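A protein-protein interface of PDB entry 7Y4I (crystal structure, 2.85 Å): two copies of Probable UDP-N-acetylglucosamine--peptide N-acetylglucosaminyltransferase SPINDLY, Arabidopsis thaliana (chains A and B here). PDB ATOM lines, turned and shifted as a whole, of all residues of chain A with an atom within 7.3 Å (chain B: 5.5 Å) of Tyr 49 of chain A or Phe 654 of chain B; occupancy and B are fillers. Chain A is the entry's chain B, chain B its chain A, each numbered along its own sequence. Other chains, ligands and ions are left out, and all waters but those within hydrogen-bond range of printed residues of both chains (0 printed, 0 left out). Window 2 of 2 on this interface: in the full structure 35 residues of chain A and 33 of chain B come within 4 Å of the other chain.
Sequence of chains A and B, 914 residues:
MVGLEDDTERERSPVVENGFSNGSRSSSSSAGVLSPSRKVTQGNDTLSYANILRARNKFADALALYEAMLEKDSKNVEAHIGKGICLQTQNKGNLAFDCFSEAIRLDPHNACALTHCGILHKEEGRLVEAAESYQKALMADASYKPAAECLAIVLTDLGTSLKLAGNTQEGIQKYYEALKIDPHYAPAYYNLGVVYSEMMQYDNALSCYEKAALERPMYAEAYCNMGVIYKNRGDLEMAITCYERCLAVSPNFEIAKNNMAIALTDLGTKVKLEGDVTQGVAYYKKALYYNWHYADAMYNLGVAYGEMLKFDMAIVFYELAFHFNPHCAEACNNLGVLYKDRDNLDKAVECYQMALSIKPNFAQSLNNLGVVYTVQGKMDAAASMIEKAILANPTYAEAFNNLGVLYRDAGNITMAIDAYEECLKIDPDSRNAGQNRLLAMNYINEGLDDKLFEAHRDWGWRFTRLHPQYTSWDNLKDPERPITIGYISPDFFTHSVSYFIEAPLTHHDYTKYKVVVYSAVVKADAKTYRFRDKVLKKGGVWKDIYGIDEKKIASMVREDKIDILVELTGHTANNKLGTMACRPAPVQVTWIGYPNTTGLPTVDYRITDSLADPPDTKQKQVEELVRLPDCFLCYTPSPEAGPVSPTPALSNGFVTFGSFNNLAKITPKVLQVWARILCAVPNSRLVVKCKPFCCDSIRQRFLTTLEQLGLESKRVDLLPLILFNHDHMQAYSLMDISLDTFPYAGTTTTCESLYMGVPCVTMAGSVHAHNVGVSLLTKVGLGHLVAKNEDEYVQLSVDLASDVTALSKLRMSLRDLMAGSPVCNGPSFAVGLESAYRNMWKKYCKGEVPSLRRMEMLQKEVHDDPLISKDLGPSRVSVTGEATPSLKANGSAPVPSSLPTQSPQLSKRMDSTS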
ATOM      1  N   TYR A  49     -16.089 -23.225  33.230  1.00  0.00           N
ATOM      2  CA  TYR A  49     -15.002 -23.152  32.262  1.00  0.00           C
ATOM      3  C   TYR A  49     -13.682 -22.831  32.954  1.00  0.00           C
ATOM      4  O   TYR A  49     -12.695 -23.544  32.770  1.00  0.00           O
ATOM      5  CB  TYR A  49     -15.307 -22.100  31.188  1.00  0.00           C
ATOM      6  CG  TYR A  49     -14.394 -22.147  29.978  1.00  0.00           C
ATOM      7  CD1 TYR A  49     -14.062 -23.355  29.373  1.00  0.00           C
ATOM      8  CD2 TYR A  49     -13.874 -20.978  29.432  1.00  0.00           C
ATOM      9  CE1 TYR A  49     -13.233 -23.398  28.264  1.00  0.00           C
ATOM     10  CE2 TYR A  49     -13.044 -21.012  28.324  1.00  0.00           C
ATOM     11  CZ  TYR A  49     -12.727 -22.224  27.746  1.00  0.00           C
ATOM     12  OH  TYR A  49     -11.902 -22.261  26.645  1.00  0.00           O
ATOM     13  N   ALA A  50     -13.711 -21.777  33.779  1.00  0.00           N
ATOM     14  CA  ALA A  50     -12.497 -21.177  34.331  1.00  0.00           C
ATOM     15  C   ALA A  50     -11.535 -22.213  34.901  1.00  0.00           C
ATOM     16  O   ALA A  50     -10.344 -22.226  34.562  1.00  0.00           O
ATOM     17  CB  ALA A  50     -12.872 -20.156  35.406  1.00  0.00           C
ATOM     18  N   ASN A  51     -12.031 -23.101  35.763  1.00  0.00           N
ATOM     19  CA  ASN A  51     -11.144 -24.018  36.468  1.00  0.00           C
ATOM     20  C   ASN A  51     -10.665 -25.164  35.591  1.00  0.00           C
ATOM     21  O   ASN A  51      -9.662 -25.805  35.927  1.00  0.00           O
ATOM     22  CB  ASN A  51     -11.835 -24.570  37.716  1.00  0.00           C
ATOM     23  CG  ASN A  51     -11.484 -23.787  38.967  1.00  0.00           C
ATOM     24  OD1 ASN A  51     -11.323 -22.566  38.923  1.00  0.00           O
ATOM     25  ND2 ASN A  51     -11.359 -24.486  40.089  1.00  0.00           N
ATOM     26  N   ILE A  52     -11.349 -25.441  34.480  1.00  0.00           N
ATOM     27  CA  ILE A  52     -10.868 -26.474  33.572  1.00  0.00           C
ATOM     28  C   ILE A  52      -9.608 -26.007  32.850  1.00  0.00           C
ATOM     29  O   ILE A  52      -8.652 -26.775  32.694  1.00  0.00           O
ATOM     30  CB  ILE A  52     -11.979 -26.883  32.586  1.00  0.00           C
ATOM     31  CG1 ILE A  52     -13.098 -27.616  33.327  1.00  0.00           C
ATOM     32  CG2 ILE A  52     -11.422 -27.757  31.473  1.00  0.00           C
ATOM     33  CD1 ILE A  52     -14.289 -27.949  32.459  1.00  0.00           C
ATOM     34  N   LEU A  53      -9.575 -24.742  32.413  1.00  0.00           N
ATOM     35  CA  LEU A  53      -8.335 -24.203  31.859  1.00  0.00           C
ATOM     36  C   LEU A  53      -7.218 -24.208  32.894  1.00  0.00           C
ATOM     37  O   LEU A  53      -6.048 -24.416  32.552  1.00  0.00           O
ATOM     38  CB  LEU A  53      -8.537 -22.783  31.323  1.00  0.00           C
ATOM     39  CG  LEU A  53      -9.694 -22.376  30.412  1.00  0.00           C
ATOM     40  CD1 LEU A  53     -10.838 -21.783  31.203  1.00  0.00           C
ATOM     41  CD2 LEU A  53      -9.199 -21.388  29.368  1.00  0.00           C
ATOM     42  N   ARG A  54      -7.557 -23.962  34.162  1.00  0.00           N
ATOM     43  CA  ARG A  54      -6.545 -23.939  35.214  1.00  0.00           C
ATOM     44  C   ARG A  54      -5.852 -25.289  35.347  1.00  0.00           C
ATOM     45  O   ARG A  54      -4.623 -25.360  35.465  1.00  0.00           O
ATOM     46  CB  ARG A  54      -7.172 -23.530  36.545  1.00  0.00           C
ATOM     47  CG  ARG A  54      -6.149 -23.297  37.647  1.00  0.00           C
ATOM     48  CD  ARG A  54      -6.771 -22.659  38.874  1.00  0.00           C
ATOM     49  NE  ARG A  54      -7.757 -23.530  39.500  1.00  0.00           N
ATOM     50  CZ  ARG A  54      -7.458 -24.515  40.335  1.00  0.00           C
ATOM     51  NH1 ARG A  54      -6.203 -24.800  40.647  1.00  0.00           N
ATOM     52  NH2 ARG A  54      -8.441 -25.234  40.871  1.00  0.00           N
ATOM     53  N   ALA A  55      -6.632 -26.376  35.344  1.00  0.00           N
ATOM     54  CA  ALA A  55      -6.046 -27.710  35.441  1.00  0.00           C
ATOM     55  C   ALA A  55      -5.087 -27.986  34.291  1.00  0.00           C
ATOM     56  O   ALA A  55      -4.150 -28.780  34.439  1.00  0.00           O
ATOM     57  CB  ALA A  55      -7.151 -28.766  35.478  1.00  0.00           C
ATOM     58  N   ARG A  56      -5.302 -27.341  33.145  1.00  0.00           N
ATOM     59  CA  ARG A  56      -4.450 -27.478  31.974  1.00  0.00           C
ATOM     60  C   ARG A  56      -3.391 -26.378  31.892  1.00  0.00           C
ATOM     61  O   ARG A  56      -2.843 -26.132  30.811  1.00  0.00           O
ATOM     62  CB  ARG A  56      -5.316 -27.516  30.714  1.00  0.00           C
ATOM     63  CG  ARG A  56      -6.458 -28.526  30.830  1.00  0.00           C
ATOM     64  CD  ARG A  56      -7.702 -28.110  30.060  1.00  0.00           C
ATOM     65  NE  ARG A  56      -8.756 -29.117  30.148  1.00  0.00           N
ATOM     66  CZ  ARG A  56      -8.921 -30.115  29.291  1.00  0.00           C
ATOM     67  NH1 ARG A  56      -8.109 -30.284  28.260  1.00  0.00           N
ATOM     68  NH2 ARG A  56      -9.927 -30.965  29.471  1.00  0.00           N
ATOM     69  N   ASP A  61      -5.467 -16.965  31.250  1.00  0.00           N
ATOM     70  CA  ASP A  61      -6.839 -16.932  30.750  1.00  0.00           C
ATOM     71  C   ASP A  61      -7.845 -17.161  31.873  1.00  0.00           C
ATOM     72  O   ASP A  61      -8.813 -16.405  32.018  1.00  0.00           O
ATOM     73  CB  ASP A  61      -7.020 -17.972  29.645  1.00  0.00           C
ATOM     74  CG  ASP A  61      -5.791 -18.109  28.768  1.00  0.00           C
ATOM     75  OD1 ASP A  61      -5.588 -17.248  27.886  1.00  0.00           O
ATOM     76  OD2 ASP A  61      -5.025 -19.077  28.966  1.00  0.00           O
ATOM     77  N   ALA A  62      -7.627 -18.206  32.679  1.00  0.00           N
ATOM     78  CA  ALA A  62      -8.536 -18.504  33.782  1.00  0.00           C
ATOM     79  C   ALA A  62      -8.547 -17.377  34.806  1.00  0.00           C
ATOM     80  O   ALA A  62      -9.605 -17.031  35.345  1.00  0.00           O
ATOM     81  CB  ALA A  62      -8.146 -19.826  34.443  1.00  0.00           C
ATOM     82  N   LEU A  65     -11.052 -14.767  33.824  1.00  0.00           N
ATOM     83  CA  LEU A  65     -12.445 -15.121  34.095  1.00  0.00           C
ATOM     84  C   LEU A  65     -12.772 -14.977  35.577  1.00  0.00           C
ATOM     85  O   LEU A  65     -13.882 -14.567  35.934  1.00  0.00           O
ATOM     86  CB  LEU A  65     -12.738 -16.542  33.605  1.00  0.00           C
ATOM     87  CG  LEU A  65     -14.200 -17.010  33.622  1.00  0.00           C
ATOM     88  CD1 LEU A  65     -15.148 -15.907  33.171  1.00  0.00           C
ATOM     89  CD2 LEU A  65     -14.375 -18.246  32.751  1.00  0.00           C
ATOM     90  N   TYR A  66     -11.820 -15.314  36.453  1.00  0.00           N
ATOM     91  CA  TYR A  66     -11.998 -15.060  37.879  1.00  0.00           C
ATOM     92  C   TYR A  66     -12.221 -13.577  38.144  1.00  0.00           C
ATOM     93  O   TYR A  66     -13.207 -13.190  38.783  1.00  0.00           O
ATOM     94  CB  TYR A  66     -10.783 -15.554  38.664  1.00  0.00           C
ATOM     95  CG  TYR A  66     -10.467 -17.024  38.513  1.00  0.00           C
ATOM     96  CD1 TYR A  66     -11.474 -17.979  38.539  1.00  0.00           C
ATOM     97  CD2 TYR A  66      -9.155 -17.458  38.362  1.00  0.00           C
ATOM     98  CE1 TYR A  66     -11.185 -19.325  38.409  1.00  0.00           C
ATOM     99  CE2 TYR A  66      -8.856 -18.798  38.227  1.00  0.00           C
ATOM    100  CZ  TYR A  66      -9.874 -19.728  38.254  1.00  0.00           C
ATOM    101  OH  TYR A  66      -9.581 -21.065  38.124  1.00  0.00           O
ATOM    102  N   MET A  69     -15.432 -12.770  37.165  1.00  0.00           N
ATOM    103  CA  MET A  69     -16.410 -13.412  38.039  1.00  0.00           C
ATOM    104  C   MET A  69     -16.593 -12.635  39.337  1.00  0.00           C
ATOM    105  O   MET A  69     -17.705 -12.565  39.876  1.00  0.00           O
ATOM    106  CB  MET A  69     -15.973 -14.847  38.333  1.00  0.00           C
ATOM    107  CG  MET A  69     -16.521 -15.889  37.370  1.00  0.00           C
ATOM    108  SD  MET A  69     -16.354 -17.563  38.017  1.00  0.00           S
ATOM    109  CE  MET A  69     -16.629 -18.537  36.540  1.00  0.00           C
ATOM    110  N   PRO B 648     -15.856 -37.354  27.766  1.00  0.00           N
ATOM    111  CA  PRO B 648     -15.738 -36.217  28.692  1.00  0.00           C
ATOM    112  C   PRO B 648     -16.587 -35.011  28.321  1.00  0.00           C
ATOM    113  O   PRO B 648     -16.645 -34.060  29.113  1.00  0.00           O
ATOM    114  CB  PRO B 648     -14.245 -35.874  28.629  1.00  0.00           C
ATOM    115  CG  PRO B 648     -13.824 -36.332  27.271  1.00  0.00           C
ATOM    116  CD  PRO B 648     -14.603 -37.598  27.031  1.00  0.00           C
ATOM    117  N   ALA B 649     -17.238 -35.011  27.154  1.00  0.00           N
ATOM    118  CA  ALA B 649     -18.036 -33.856  26.752  1.00  0.00           C
ATOM    119  C   ALA B 649     -19.204 -33.612  27.700  1.00  0.00           C
ATOM    120  O   ALA B 649     -19.618 -32.462  27.890  1.00  0.00           O
ATOM    121  CB  ALA B 649     -18.544 -34.039  25.321  1.00  0.00           C
ATOM    122  N   ASN B 652     -17.509 -31.803  30.718  1.00  0.00           N
ATOM    123  CA  ASN B 652     -16.840 -30.539  30.428  1.00  0.00           C
ATOM    124  C   ASN B 652     -17.816 -29.470  29.954  1.00  0.00           C
ATOM    125  O   ASN B 652     -17.661 -28.291  30.292  1.00  0.00           O
ATOM    126  CB  ASN B 652     -15.752 -30.754  29.380  1.00  0.00           C
ATOM    127  CG  ASN B 652     -14.560 -31.508  29.924  1.00  0.00           C
ATOM    128  OD1 ASN B 652     -13.694 -30.933  30.581  1.00  0.00           O
ATOM    129  ND2 ASN B 652     -14.511 -32.806  29.656  1.00  0.00           N
ATOM    130  N   GLY B 653     -18.825 -29.857  29.178  1.00  0.00           N
ATOM    131  CA  GLY B 653     -19.645 -28.897  28.478  1.00  0.00           C
ATOM    132  C   GLY B 653     -19.135 -28.527  27.104  1.00  0.00           C
ATOM    133  O   GLY B 653     -19.809 -27.766  26.395  1.00  0.00           O
ATOM    134  N   PHE B 654     -17.964 -29.027  26.712  1.00  0.00           N
ATOM    135  CA  PHE B 654     -17.429 -28.807  25.377  1.00  0.00           C
ATOM    136  C   PHE B 654     -16.848 -30.107  24.838  1.00  0.00           C
ATOM    137  O   PHE B 654     -16.520 -31.027  25.591  1.00  0.00           O
ATOM    138  CB  PHE B 654     -16.365 -27.701  25.358  1.00  0.00           C
ATOM    139  CG  PHE B 654     -15.347 -27.793  26.462  1.00  0.00           C
ATOM    140  CD1 PHE B 654     -14.404 -28.809  26.478  1.00  0.00           C
ATOM    141  CD2 PHE B 654     -15.313 -26.838  27.467  1.00  0.00           C
ATOM    142  CE1 PHE B 654     -13.465 -28.886  27.489  1.00  0.00           C
ATOM    143  CE2 PHE B 654     -14.375 -26.908  28.479  1.00  0.00           C
ATOM    144  CZ  PHE B 654     -13.449 -27.933  28.490  1.00  0.00           C
ATOM    145  N   VAL B 655     -16.730 -30.170  23.519  1.00  0.00           N
ATOM    146  CA  VAL B 655     -16.167 -31.332  22.842  1.00  0.00           C
ATOM    147  C   VAL B 655     -14.667 -31.125  22.681  1.00  0.00           C
ATOM    148  O   VAL B 655     -14.208 -30.032  22.332  1.00  0.00           O
ATOM    149  CB  VAL B 655     -16.854 -31.556  21.482  1.00  0.00           C
ATOM    150  CG1 VAL B 655     -16.303 -32.801  20.798  1.00  0.00           C
ATOM    151  CG2 VAL B 655     -18.366 -31.656  21.665  1.00  0.00           C
ATOM    152  N   THR B 656     -13.899 -32.175  22.950  1.00  0.00           N
ATOM    153  CA  THR B 656     -12.447 -32.145  22.847  1.00  0.00           C
ATOM    154  C   THR B 656     -12.007 -32.943  21.628  1.00  0.00           C
ATOM    155  O   THR B 656     -12.418 -34.095  21.453  1.00  0.00           O
ATOM    156  CB  THR B 656     -11.797 -32.714  24.110  1.00  0.00           C
ATOM    157  OG1 THR B 656     -12.137 -34.099  24.234  1.00  0.00           O
ATOM    158  CG2 THR B 656     -12.289 -31.968  25.348  1.00  0.00           C
ATOM    159  N   ASN B 683     -16.232 -23.117  20.950  1.00  0.00           N
ATOM    160  CA  ASN B 683     -15.895 -23.394  22.342  1.00  0.00           C
ATOM    161  C   ASN B 683     -15.454 -24.842  22.533  1.00  0.00           C
ATOM    162  O   ASN B 683     -15.806 -25.493  23.513  1.00  0.00           O
ATOM    163  CB  ASN B 683     -17.067 -23.055  23.264  1.00  0.00           C
ATOM    164  CG  ASN B 683     -17.259 -21.564  23.430  1.00  0.00           C
ATOM    165  OD1 ASN B 683     -18.028 -20.940  22.700  1.00  0.00           O
ATOM    166  ND2 ASN B 683     -16.556 -20.981  24.395  1.00  0.00           N
ATOM    167  N   SER B 684     -14.669 -25.350  21.588  1.00  0.00           N
ATOM    168  CA  SER B 684     -14.083 -26.676  21.682  1.00  0.00           C
ATOM    169  C   SER B 684     -12.571 -26.527  21.728  1.00  0.00           C
ATOM    170  O   SER B 684     -12.023 -25.482  21.370  1.00  0.00           O
ATOM    171  CB  SER B 684     -14.488 -27.567  20.498  1.00  0.00           C
ATOM    172  OG  SER B 684     -14.176 -26.959  19.257  1.00  0.00           O
ATOM    173  N   ARG B 685     -11.890 -27.579  22.168  1.00  0.00           N
ATOM    174  CA  ARG B 685     -10.459 -27.478  22.378  1.00  0.00           C
ATOM    175  C   ARG B 685      -9.722 -28.642  21.732  1.00  0.00           C
ATOM    176  O   ARG B 685     -10.295 -29.694  21.433  1.00  0.00           O
ATOM    177  CB  ARG B 685     -10.117 -27.391  23.871  1.00  0.00           C
ATOM    178  CG  ARG B 685     -10.533 -28.581  24.716  1.00  0.00           C
ATOM    179  CD  ARG B 685     -10.327 -28.292  26.201  1.00  0.00           C
ATOM    180  NE  ARG B 685      -9.100 -27.548  26.471  1.00  0.00           N
ATOM    181  CZ  ARG B 685      -9.042 -26.234  26.650  1.00  0.00           C
ATOM    182  NH1 ARG B 685     -10.126 -25.478  26.572  1.00  0.00           N
ATOM    183  NH2 ARG B 685      -7.865 -25.664  26.896  1.00  0.00           N
ATOM    184  N   LYS B 714      -5.615 -20.509  24.160  1.00  0.00           N
ATOM    185  CA  LYS B 714      -6.417 -20.994  25.280  1.00  0.00           C
ATOM    186  C   LYS B 714      -7.272 -22.200  24.912  1.00  0.00           C
ATOM    187  O   LYS B 714      -7.779 -22.881  25.812  1.00  0.00           O
ATOM    188  CB  LYS B 714      -7.295 -19.866  25.832  1.00  0.00           C
ATOM    189  CG  LYS B 714      -8.695 -19.795  25.245  1.00  0.00           C
ATOM    190  CD  LYS B 714      -9.465 -18.609  25.808  1.00  0.00           C
ATOM    191  CE  LYS B 714      -8.708 -17.305  25.599  1.00  0.00           C
ATOM    192  NZ  LYS B 714      -9.117 -16.253  26.571  1.00  0.00           N
ATOM    193  N   ARG B 715      -7.448 -22.482  23.621  1.00  0.00           N
ATOM    194  CA  ARG B 715      -8.237 -23.616  23.162  1.00  0.00           C
ATOM    195  C   ARG B 715      -7.383 -24.803  22.730  1.00  0.00           C
ATOM    196  O   ARG B 715      -7.900 -25.721  22.087  1.00  0.00           O
ATOM    197  CB  ARG B 715      -9.156 -23.187  22.019  1.00  0.00           C
ATOM    198  CG  ARG B 715     -10.217 -22.185  22.424  1.00  0.00           C
ATOM    199  CD  ARG B 715     -11.158 -21.864  21.273  1.00  0.00           C
ATOM    200  NE  ARG B 715     -11.874 -23.046  20.808  1.00  0.00           N
ATOM    201  CZ  ARG B 715     -12.526 -23.126  19.656  1.00  0.00           C
ATOM    202  NH1 ARG B 715     -12.625 -22.086  18.844  1.00  0.00           N
ATOM    203  NH2 ARG B 715     -13.099 -24.275  19.314  1.00  0.00           N
ATOM    204  N   ASP B 736     -12.678 -36.702  23.163  1.00  0.00           N
ATOM    205  CA  ASP B 736     -13.927 -37.299  22.689  1.00  0.00           C
ATOM    206  C   ASP B 736     -13.763 -37.959  21.326  1.00  0.00           C
ATOM    207  O   ASP B 736     -14.300 -39.048  21.095  1.00  0.00           O
ATOM    208  CB  ASP B 736     -15.041 -36.252  22.593  1.00  0.00           C
ATOM    209  CG  ASP B 736     -15.114 -35.338  23.798  1.00  0.00           C
ATOM    210  OD1 ASP B 736     -14.645 -34.189  23.700  1.00  0.00           O
ATOM    211  OD2 ASP B 736     -15.689 -35.745  24.826  1.00  0.00           O
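NE of Arg 685 of chain B sits close to NH1 of Arg 56 of chain A, 3.4 Å away.
NZ of Lys 714 of chain B lies within salt-bridge range of OD1 of Asp 61 of chain A, 3.9 Å away.
The backbone carbonyl oxygen (O) of Lys 714 of chain B sits at hydrogen-bond distance from the guanidinium group (NH2) of Arg 685 of chain B (3.0 Å).
The backbone carbonyl oxygen of Val 655 of chain B lies within hydrogen-bond range of the backbone NH of Arg 685 of chain B (3.4 Å).
The backbone carbonyl oxygen (O) of Ile 52 of chain A lies close to the guanidinium group (NE) of Arg 56 of chain A, 3.5 Å away.
The backbone carbonyl oxygen (O) of Pro 648 of chain B sits at hydrogen-bond distance from the side-chain amide nitrogen (ND2) of Asn 652 of chain B (2.5 Å).
Among the printed residues, pairs that only touch across the chains: Tyr 49 of chain A with Phe 654 of chain B, Tyr 49 of chain A with Arg 685 of chain B, Ile 52 of chain A with Asn 652 of chain B, Ile 52 of chain A with Phe 654 of chain B and Arg 56 of chain A with Asn 652 of chain B.
Of chain B, only Phe 654 and Arg 685 come within 4 Å of Tyr 49 of chain A.
Of chain A, only Tyr 49 (3.7 Å) and Ile 52 (3.6 Å) come within 4 Å of Phe 654 of chain B.
No residue of chain A comes within 4 Å of Gly 653 of chain B.
Of the printed residues of chain A, Lys 714 of chain B touches Asp 61 (3.7 Å).
Printed residues of chain B within 4 Å of Asp 61 of chain A: Lys 714.
Of the printed residues of chain A, Asn 652 of chain B touches Ile 52 and Arg 56.
Printed residues of chain A within 4 Å of Arg 685 of chain B: Tyr 49 and Arg 56.
Printed residues of chain B within 4 Å of Arg 56 of chain A: Asn 652 (3.9 Å) and Arg 685 (3.4 Å).
Met 69 of chain A touches none of the printed residues of chain B.
Val 655 of chain B touches none of the printed residues of chain A.
The nearest residue of chain A that does not touch Phe 654 of chain B is Arg 56 of chain A (4.6 Å).
The nearest printed residue of chain B that does not touch Asp 61 of chain A is Arg 715 of chain B (6.8 Å).
Along chain A the printed residues that touch a printed residue of chain B span positions 49 to 61.
Printed residues of chain B that touch a printed residue of chain A: Asn 652, Phe 654, Arg 685 and Lys 714.
Hydrophobic or aromatic side chains of chain B within 4 Å of the printed part of chain A: Phe 654.
Along chain B the printed residues that touch a printed residue of chain A span positions 652 to 714.
Among the printed residues, 7 pairs touch across the chains.
Among the printed residues, Asp or Glu carboxylates within 4 Å of a Lys or Arg side-chain nitrogen of the other chain: Asp 61 of chain A with Lys 714 of chain B (3.9 Å).
No position is printed for both chains.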
